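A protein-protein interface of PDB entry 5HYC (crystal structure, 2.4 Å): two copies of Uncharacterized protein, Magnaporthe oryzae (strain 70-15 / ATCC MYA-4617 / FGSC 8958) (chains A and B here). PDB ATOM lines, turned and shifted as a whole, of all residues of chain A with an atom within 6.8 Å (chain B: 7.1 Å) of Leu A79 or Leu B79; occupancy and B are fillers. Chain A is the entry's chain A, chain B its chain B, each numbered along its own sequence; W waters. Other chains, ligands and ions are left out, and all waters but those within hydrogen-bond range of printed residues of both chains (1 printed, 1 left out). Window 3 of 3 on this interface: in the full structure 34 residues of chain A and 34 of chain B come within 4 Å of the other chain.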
ATOM      1  N   GLN A  77     -17.262   0.167  31.543  1.00  0.00           N
ATOM      2  CA  GLN A  77     -18.108  -0.178  30.426  1.00  0.00           C
ATOM      3  C   GLN A  77     -17.478  -1.276  29.536  1.00  0.00           C
ATOM      4  O   GLN A  77     -16.275  -1.339  29.334  1.00  0.00           O
ATOM      5  CB  GLN A  77     -18.423   1.060  29.597  1.00  0.00           C
ATOM      6  CG  GLN A  77     -19.574   0.847  28.660  1.00  0.00           C
ATOM      7  CD  GLN A  77     -19.845   2.028  27.779  1.00  0.00           C
ATOM      8  OE1 GLN A  77     -18.969   2.842  27.554  1.00  0.00           O
ATOM      9  NE2 GLN A  77     -21.061   2.122  27.261  1.00  0.00           N
ATOM     10  N   HIS A  78     -18.327  -2.170  29.057  1.00  0.00           N
ATOM     11  CA  HIS A  78     -17.946  -3.129  28.033  1.00  0.00           C
ATOM     12  C   HIS A  78     -17.665  -2.410  26.715  1.00  0.00           C
ATOM     13  O   HIS A  78     -18.133  -1.297  26.493  1.00  0.00           O
ATOM     14  CB  HIS A  78     -19.044  -4.163  27.840  1.00  0.00           C
ATOM     15  CG  HIS A  78     -19.235  -5.070  29.011  1.00  0.00           C
ATOM     16  ND1 HIS A  78     -20.325  -5.900  29.135  1.00  0.00           N
ATOM     17  CD2 HIS A  78     -18.482  -5.271  30.116  1.00  0.00           C
ATOM     18  CE1 HIS A  78     -20.230  -6.581  30.258  1.00  0.00           C
ATOM     19  NE2 HIS A  78     -19.126  -6.209  30.877  1.00  0.00           N
ATOM     20  N   LEU A  79     -16.907  -3.058  25.843  1.00  0.00           N
ATOM     21  CA  LEU A  79     -16.698  -2.537  24.498  1.00  0.00           C
ATOM     22  C   LEU A  79     -18.021  -2.516  23.749  1.00  0.00           C
ATOM     23  O   LEU A  79     -18.848  -3.385  23.918  1.00  0.00           O
ATOM     24  CB  LEU A  79     -15.655  -3.354  23.750  1.00  0.00           C
ATOM     25  CG  LEU A  79     -14.251  -3.350  24.351  1.00  0.00           C
ATOM     26  CD1 LEU A  79     -13.278  -4.143  23.488  1.00  0.00           C
ATOM     27  CD2 LEU A  79     -13.756  -1.938  24.538  1.00  0.00           C
ATOM     28  N   VAL A  80     -18.219  -1.464  22.980  1.00  0.00           N
ATOM     29  CA  VAL A  80     -19.440  -1.210  22.231  1.00  0.00           C
ATOM     30  C   VAL A  80     -19.162  -1.505  20.757  1.00  0.00           C
ATOM     31  O   VAL A  80     -18.162  -1.044  20.210  1.00  0.00           O
ATOM     32  CB  VAL A  80     -19.913   0.264  22.411  1.00  0.00           C
ATOM     33  CG1 VAL A  80     -21.228   0.516  21.709  1.00  0.00           C
ATOM     34  CG2 VAL A  80     -19.980   0.635  23.904  1.00  0.00           C
ATOM     35  N   PRO A  81     -20.004  -2.321  20.123  1.00  0.00           N
ATOM     36  CA  PRO A  81     -19.743  -2.612  18.707  1.00  0.00           C
ATOM     37  C   PRO A  81     -19.796  -1.370  17.846  1.00  0.00           C
ATOM     38  O   PRO A  81     -20.486  -0.407  18.179  1.00  0.00           O
ATOM     39  CB  PRO A  81     -20.863  -3.591  18.329  1.00  0.00           C
ATOM     40  CG  PRO A  81     -21.871  -3.474  19.421  1.00  0.00           C
ATOM     41  CD  PRO A  81     -21.117  -3.119  20.657  1.00  0.00           C
ATOM     42  N   VAL A 109     -18.528 -10.937  25.411  1.00  0.00           N
ATOM     43  CA  VAL A 109     -18.262  -9.612  25.937  1.00  0.00           C
ATOM     44  C   VAL A 109     -16.891  -9.114  25.472  1.00  0.00           C
ATOM     45  O   VAL A 109     -15.884  -9.763  25.688  1.00  0.00           O
ATOM     46  CB  VAL A 109     -18.347  -9.608  27.480  1.00  0.00           C
ATOM     47  CG1 VAL A 109     -17.960  -8.253  28.035  1.00  0.00           C
ATOM     48  CG2 VAL A 109     -19.752 -10.005  27.939  1.00  0.00           C
ATOM     49  N   GLY A 110     -16.867  -7.972  24.801  1.00  0.00           N
ATOM     50  CA  GLY A 110     -15.612  -7.298  24.537  1.00  0.00           C
ATOM     51  C   GLY A 110     -15.194  -6.465  25.745  1.00  0.00           C
ATOM     52  O   GLY A 110     -15.989  -5.737  26.309  1.00  0.00           O
ATOM     53  N   ARG A 111     -13.943  -6.611  26.149  1.00  0.00           N
ATOM     54  CA  ARG A 111     -13.370  -5.824  27.217  1.00  0.00           C
ATOM     55  C   ARG A 111     -12.033  -5.249  26.832  1.00  0.00           C
ATOM     56  O   ARG A 111     -11.214  -5.905  26.198  1.00  0.00           O
ATOM     57  CB  ARG A 111     -13.202  -6.658  28.484  1.00  0.00           C
ATOM     58  CG  ARG A 111     -14.500  -7.075  29.125  1.00  0.00           C
ATOM     59  CD  ARG A 111     -14.260  -7.920  30.362  1.00  0.00           C
ATOM     60  NE  ARG A 111     -15.517  -8.226  31.023  1.00  0.00           N
ATOM     61  CZ  ARG A 111     -16.201  -9.362  30.883  1.00  0.00           C
ATOM     62  NH1 ARG A 111     -15.756 -10.343  30.104  1.00  0.00           N
ATOM     63  NH2 ARG A 111     -17.346  -9.515  31.528  1.00  0.00           N
ATOM     64  N   ARG A 112     -11.810  -4.007  27.233  1.00  0.00           N
ATOM     65  CA  ARG A 112     -10.490  -3.431  27.181  1.00  0.00           C
ATOM     66  C   ARG A 112      -9.569  -4.139  28.186  1.00  0.00           C
ATOM     67  O   ARG A 112     -10.025  -4.708  29.166  1.00  0.00           O
ATOM     68  CB  ARG A 112     -10.572  -1.937  27.456  1.00  0.00           C
ATOM     69  CG  ARG A 112     -10.976  -1.596  28.879  1.00  0.00           C
ATOM     70  CD  ARG A 112     -10.715  -0.163  29.206  1.00  0.00           C
ATOM     71  NE  ARG A 112     -11.833   0.734  29.015  1.00  0.00           N
ATOM     72  CZ  ARG A 112     -11.702   2.048  28.838  1.00  0.00           C
ATOM     73  NH1 ARG A 112     -10.496   2.594  28.731  1.00  0.00           N
ATOM     74  NH2 ARG A 112     -12.779   2.811  28.724  1.00  0.00           N
ATOM     75  N   GLY A 113      -8.267  -4.114  27.939  1.00  0.00           N
ATOM     76  CA  GLY A 113      -7.344  -4.714  28.870  1.00  0.00           C
ATOM     77  C   GLY A 113      -7.113  -3.827  30.071  1.00  0.00           C
ATOM     78  O   GLY A 113      -7.081  -2.608  29.954  1.00  0.00           O
ATOM     79  N   GLY A 141     -23.611  -4.706  29.903  1.00  0.00           N
ATOM     80  CA  GLY A 141     -22.741  -3.744  29.270  1.00  0.00           C
ATOM     81  C   GLY A 141     -21.663  -3.134  30.150  1.00  0.00           C
ATOM     82  O   GLY A 141     -21.013  -2.199  29.732  1.00  0.00           O
ATOM     83  N   VAL B  76      -4.679   0.750  32.227  1.00  0.00           N
ATOM     84  CA  VAL B  76      -5.913   0.612  31.485  1.00  0.00           C
ATOM     85  C   VAL B  76      -5.670   0.883  30.014  1.00  0.00           C
ATOM     86  O   VAL B  76      -5.243   1.968  29.642  1.00  0.00           O
ATOM     87  CB  VAL B  76      -7.000   1.584  32.031  1.00  0.00           C
ATOM     88  CG1 VAL B  76      -8.318   1.365  31.338  1.00  0.00           C
ATOM     89  CG2 VAL B  76      -7.161   1.406  33.513  1.00  0.00           C
ATOM     90  N   GLN B  77      -5.952  -0.112  29.180  1.00  0.00           N
ATOM     91  CA  GLN B  77      -5.855   0.028  27.732  1.00  0.00           C
ATOM     92  C   GLN B  77      -6.840   1.075  27.196  1.00  0.00           C
ATOM     93  O   GLN B  77      -7.986   1.112  27.610  1.00  0.00           O
ATOM     94  CB  GLN B  77      -6.095  -1.338  27.064  1.00  0.00           C
ATOM     95  CG  GLN B  77      -6.113  -1.320  25.548  1.00  0.00           C
ATOM     96  CD  GLN B  77      -6.488  -2.665  24.958  1.00  0.00           C
ATOM     97  OE1 GLN B  77      -7.361  -3.358  25.470  1.00  0.00           O
ATOM     98  NE2 GLN B  77      -5.820  -3.045  23.887  1.00  0.00           N
ATOM     99  N   HIS B  78      -6.389   1.942  26.295  1.00  0.00           N
ATOM    100  CA  HIS B  78      -7.325   2.826  25.618  1.00  0.00           C
ATOM    101  C   HIS B  78      -8.356   2.074  24.764  1.00  0.00           C
ATOM    102  O   HIS B  78      -8.092   0.996  24.224  1.00  0.00           O
ATOM    103  CB  HIS B  78      -6.592   3.810  24.716  1.00  0.00           C
ATOM    104  CG  HIS B  78      -5.868   4.890  25.443  1.00  0.00           C
ATOM    105  ND1 HIS B  78      -5.064   5.803  24.801  1.00  0.00           N
ATOM    106  CD2 HIS B  78      -5.822   5.213  26.764  1.00  0.00           C
ATOM    107  CE1 HIS B  78      -4.552   6.638  25.687  1.00  0.00           C
ATOM    108  NE2 HIS B  78      -5.002   6.295  26.884  1.00  0.00           N
ATOM    109  N   LEU B  79      -9.526   2.677  24.629  1.00  0.00           N
ATOM    110  CA  LEU B  79     -10.472   2.268  23.609  1.00  0.00           C
ATOM    111  C   LEU B  79      -9.909   2.623  22.242  1.00  0.00           C
ATOM    112  O   LEU B  79      -9.239   3.636  22.093  1.00  0.00           O
ATOM    113  CB  LEU B  79     -11.829   2.941  23.809  1.00  0.00           C
ATOM    114  CG  LEU B  79     -12.532   2.722  25.145  1.00  0.00           C
ATOM    115  CD1 LEU B  79     -13.967   3.212  25.062  1.00  0.00           C
ATOM    116  CD2 LEU B  79     -12.478   1.268  25.524  1.00  0.00           C
ATOM    117  N   VAL B  80     -10.183   1.779  21.256  1.00  0.00           N
ATOM    118  CA  VAL B  80      -9.794   2.026  19.878  1.00  0.00           C
ATOM    119  C   VAL B  80     -10.298   3.409  19.465  1.00  0.00           C
ATOM    120  O   VAL B  80     -11.398   3.810  19.826  1.00  0.00           O
ATOM    121  CB  VAL B  80     -10.328   0.899  18.936  1.00  0.00           C
ATOM    122  CG1 VAL B  80     -11.822   1.026  18.701  1.00  0.00           C
ATOM    123  CG2 VAL B  80      -9.563   0.858  17.632  1.00  0.00           C
ATOM    124  N   PRO B  81      -9.457   4.181  18.772  1.00  0.00           N
ATOM    125  CA  PRO B  81      -9.880   5.547  18.440  1.00  0.00           C
ATOM    126  C   PRO B  81     -10.960   5.604  17.358  1.00  0.00           C
ATOM    127  O   PRO B  81     -11.142   4.647  16.611  1.00  0.00           O
ATOM    128  CB  PRO B  81      -8.584   6.209  17.958  1.00  0.00           C
ATOM    129  CG  PRO B  81      -7.683   5.079  17.571  1.00  0.00           C
ATOM    130  CD  PRO B  81      -8.036   3.937  18.464  1.00  0.00           C
ATOM    131  N   SER B  82     -11.681   6.720  17.299  1.00  0.00           N
ATOM    132  CA  SER B  82     -12.693   6.942  16.271  1.00  0.00           C
ATOM    133  C   SER B  82     -12.061   7.037  14.883  1.00  0.00           C
ATOM    134  O   SER B  82     -12.654   6.621  13.888  1.00  0.00           O
ATOM    135  CB  SER B  82     -13.491   8.213  16.578  1.00  0.00           C
ATOM    136  OG  SER B  82     -13.952   8.839  15.392  1.00  0.00           O
ATOM    137  N   ARG B 112     -16.067   9.016  30.394  1.00  0.00           N
ATOM    138  CA  ARG B 112     -15.959   7.959  29.411  1.00  0.00           C
ATOM    139  C   ARG B 112     -16.362   6.602  29.968  1.00  0.00           C
ATOM    140  O   ARG B 112     -17.320   6.489  30.727  1.00  0.00           O
ATOM    141  CB  ARG B 112     -14.540   7.856  28.868  1.00  0.00           C
ATOM    142  CG  ARG B 112     -13.576   8.942  29.250  1.00  0.00           C
ATOM    143  CD  ARG B 112     -12.285   8.700  28.478  1.00  0.00           C
ATOM    144  NE  ARG B 112     -12.591   8.708  27.042  1.00  0.00           N
ATOM    145  CZ  ARG B 112     -12.504   7.655  26.227  1.00  0.00           C
ATOM    146  NH1 ARG B 112     -12.076   6.482  26.673  1.00  0.00           N
ATOM    147  NH2 ARG B 112     -12.835   7.785  24.952  1.00  0.00           N
ATOM    148  N   GLY B 113     -15.592   5.579  29.597  1.00  0.00           N
ATOM    149  CA  GLY B 113     -15.962   4.196  29.837  1.00  0.00           C
ATOM    150  C   GLY B 113     -15.584   3.576  31.165  1.00  0.00           C
ATOM    151  O   GLY B 113     -15.972   2.458  31.420  1.00  0.00           O
ATOM    152  N   MET B 114     -14.800   4.246  32.001  1.00  0.00           N
ATOM    153  CA  MET B 114     -14.662   3.760  33.366  1.00  0.00           C
ATOM    154  C   MET B 114     -14.501   4.836  34.407  1.00  0.00           C
ATOM    155  O   MET B 114     -13.898   5.859  34.170  1.00  0.00           O
ATOM    156  CB  MET B 114     -13.513   2.766  33.496  1.00  0.00           C
ATOM    157  CG  MET B 114     -12.147   3.251  33.192  1.00  0.00           C
ATOM    158  SD  MET B 114     -10.941   2.127  33.945  1.00  0.00           S
ATOM    159  CE  MET B 114     -10.907   2.740  35.625  1.00  0.00           C
ATOM    160  N   GLU B 138      -3.018   9.346  22.226  1.00  0.00           N
ATOM    161  CA  GLU B 138      -3.548   8.325  21.342  1.00  0.00           C
ATOM    162  C   GLU B 138      -2.514   7.268  20.905  1.00  0.00           C
ATOM    163  O   GLU B 138      -2.827   6.092  20.828  1.00  0.00           O
ATOM    164  CB  GLU B 138      -4.169   8.987  20.119  1.00  0.00           C
ATOM    165  CG  GLU B 138      -4.645   8.001  19.064  1.00  0.00           C
ATOM    166  CD  GLU B 138      -5.290   8.685  17.877  1.00  0.00           C
ATOM    167  OE1 GLU B 138      -5.131   8.185  16.741  1.00  0.00           O
ATOM    168  OE2 GLU B 138      -5.960   9.722  18.080  1.00  0.00           O
ATOM    169  N   GLY B 141      -1.784   4.602  23.807  1.00  0.00           N
ATOM    170  CA  GLY B 141      -2.808   3.586  23.936  1.00  0.00           C
ATOM    171  C   GLY B 141      -3.108   3.034  25.316  1.00  0.00           C
ATOM    172  O   GLY B 141      -3.727   1.987  25.433  1.00  0.00           O
HETATM  173  O   HOH W   1     -14.635   1.140  28.793  1.00  0.00           O
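OE1 of Gln B77 lies within hydrogen-bond range of N of Gly A113 (2.7 Å).
NH1 of Arg A112 lies within hydrogen-bond range of O of Gln B77 (3.1 Å).
The backbone NH (N) of Gln A77 lies within hydrogen-bond range of the backbone carbonyl oxygen (O) of Gly B113 (2.6 Å).
N of Leu A79 is in hydrogen-bond range of O of Gly A110 (2.9 Å).
Among the printed residues, merely in contact across the chains: Leu A79 with Leu B79, Arg A112 with Val B76, Arg A112 with Leu B79, Arg A112 with Gly B113 and Gly A113 with Val B76.
Leu B79 touches two residues of chain A.
Of the printed residues of chain A, Val B76 touches Arg A112 (3.6 Å) and Gly A113 (3.8 Å).
Of the printed residues of chain B, Gln A77 touches Gly B113.
Of the printed residues of chain A, Gln B77 touches Arg A112 (3.1 Å) and Gly A113 (2.7 Å).
The nearest residue of chain B that does not touch Leu A79 is Val B80 (6.1 Å).
The nearest printed residue of chain B that does not touch Gly A113 is His B78 (5.9 Å).
Of the 11 printed residues of chain A, 4 touch a printed residue of chain B.
Hydrophobic or aromatic side chains of chain A that line the printed part of chain B: Leu A79.
Among the printed residues, 8 pairs touch across the chains.
Among the printed residues, no Asp or Glu carboxylate lies within 4 Å of a Lys or Arg side-chain nitrogen of the other chain.
Gln A77 touches Gly B113, and with the chains exchanged Gly A113 touches Gln B77.
Leu B79 touches its own counterpart, Leu A79.
Arg A112 touches Gln B77, but with the chains exchanged Gln A77 does not touch Arg B112 (5.1 Å).
Arg A112 touches Gly B113, but with the chains exchanged Gly A113 does not touch Arg B112 (10.9 Å).
Positions printed for both chains: 77, 78, 79, 80, 81, 112, 113 and 141.
Of the 8 pairs that touch across the chains among the printed residues, 3 have their exchanged pair printed and touching as well.
Water W1 lies within hydrogen-bond range of NH2 of Arg A112 (2.5 Å), O of Gln A77 (3.0 Å) and O of Gly B113 (3.2 Å).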
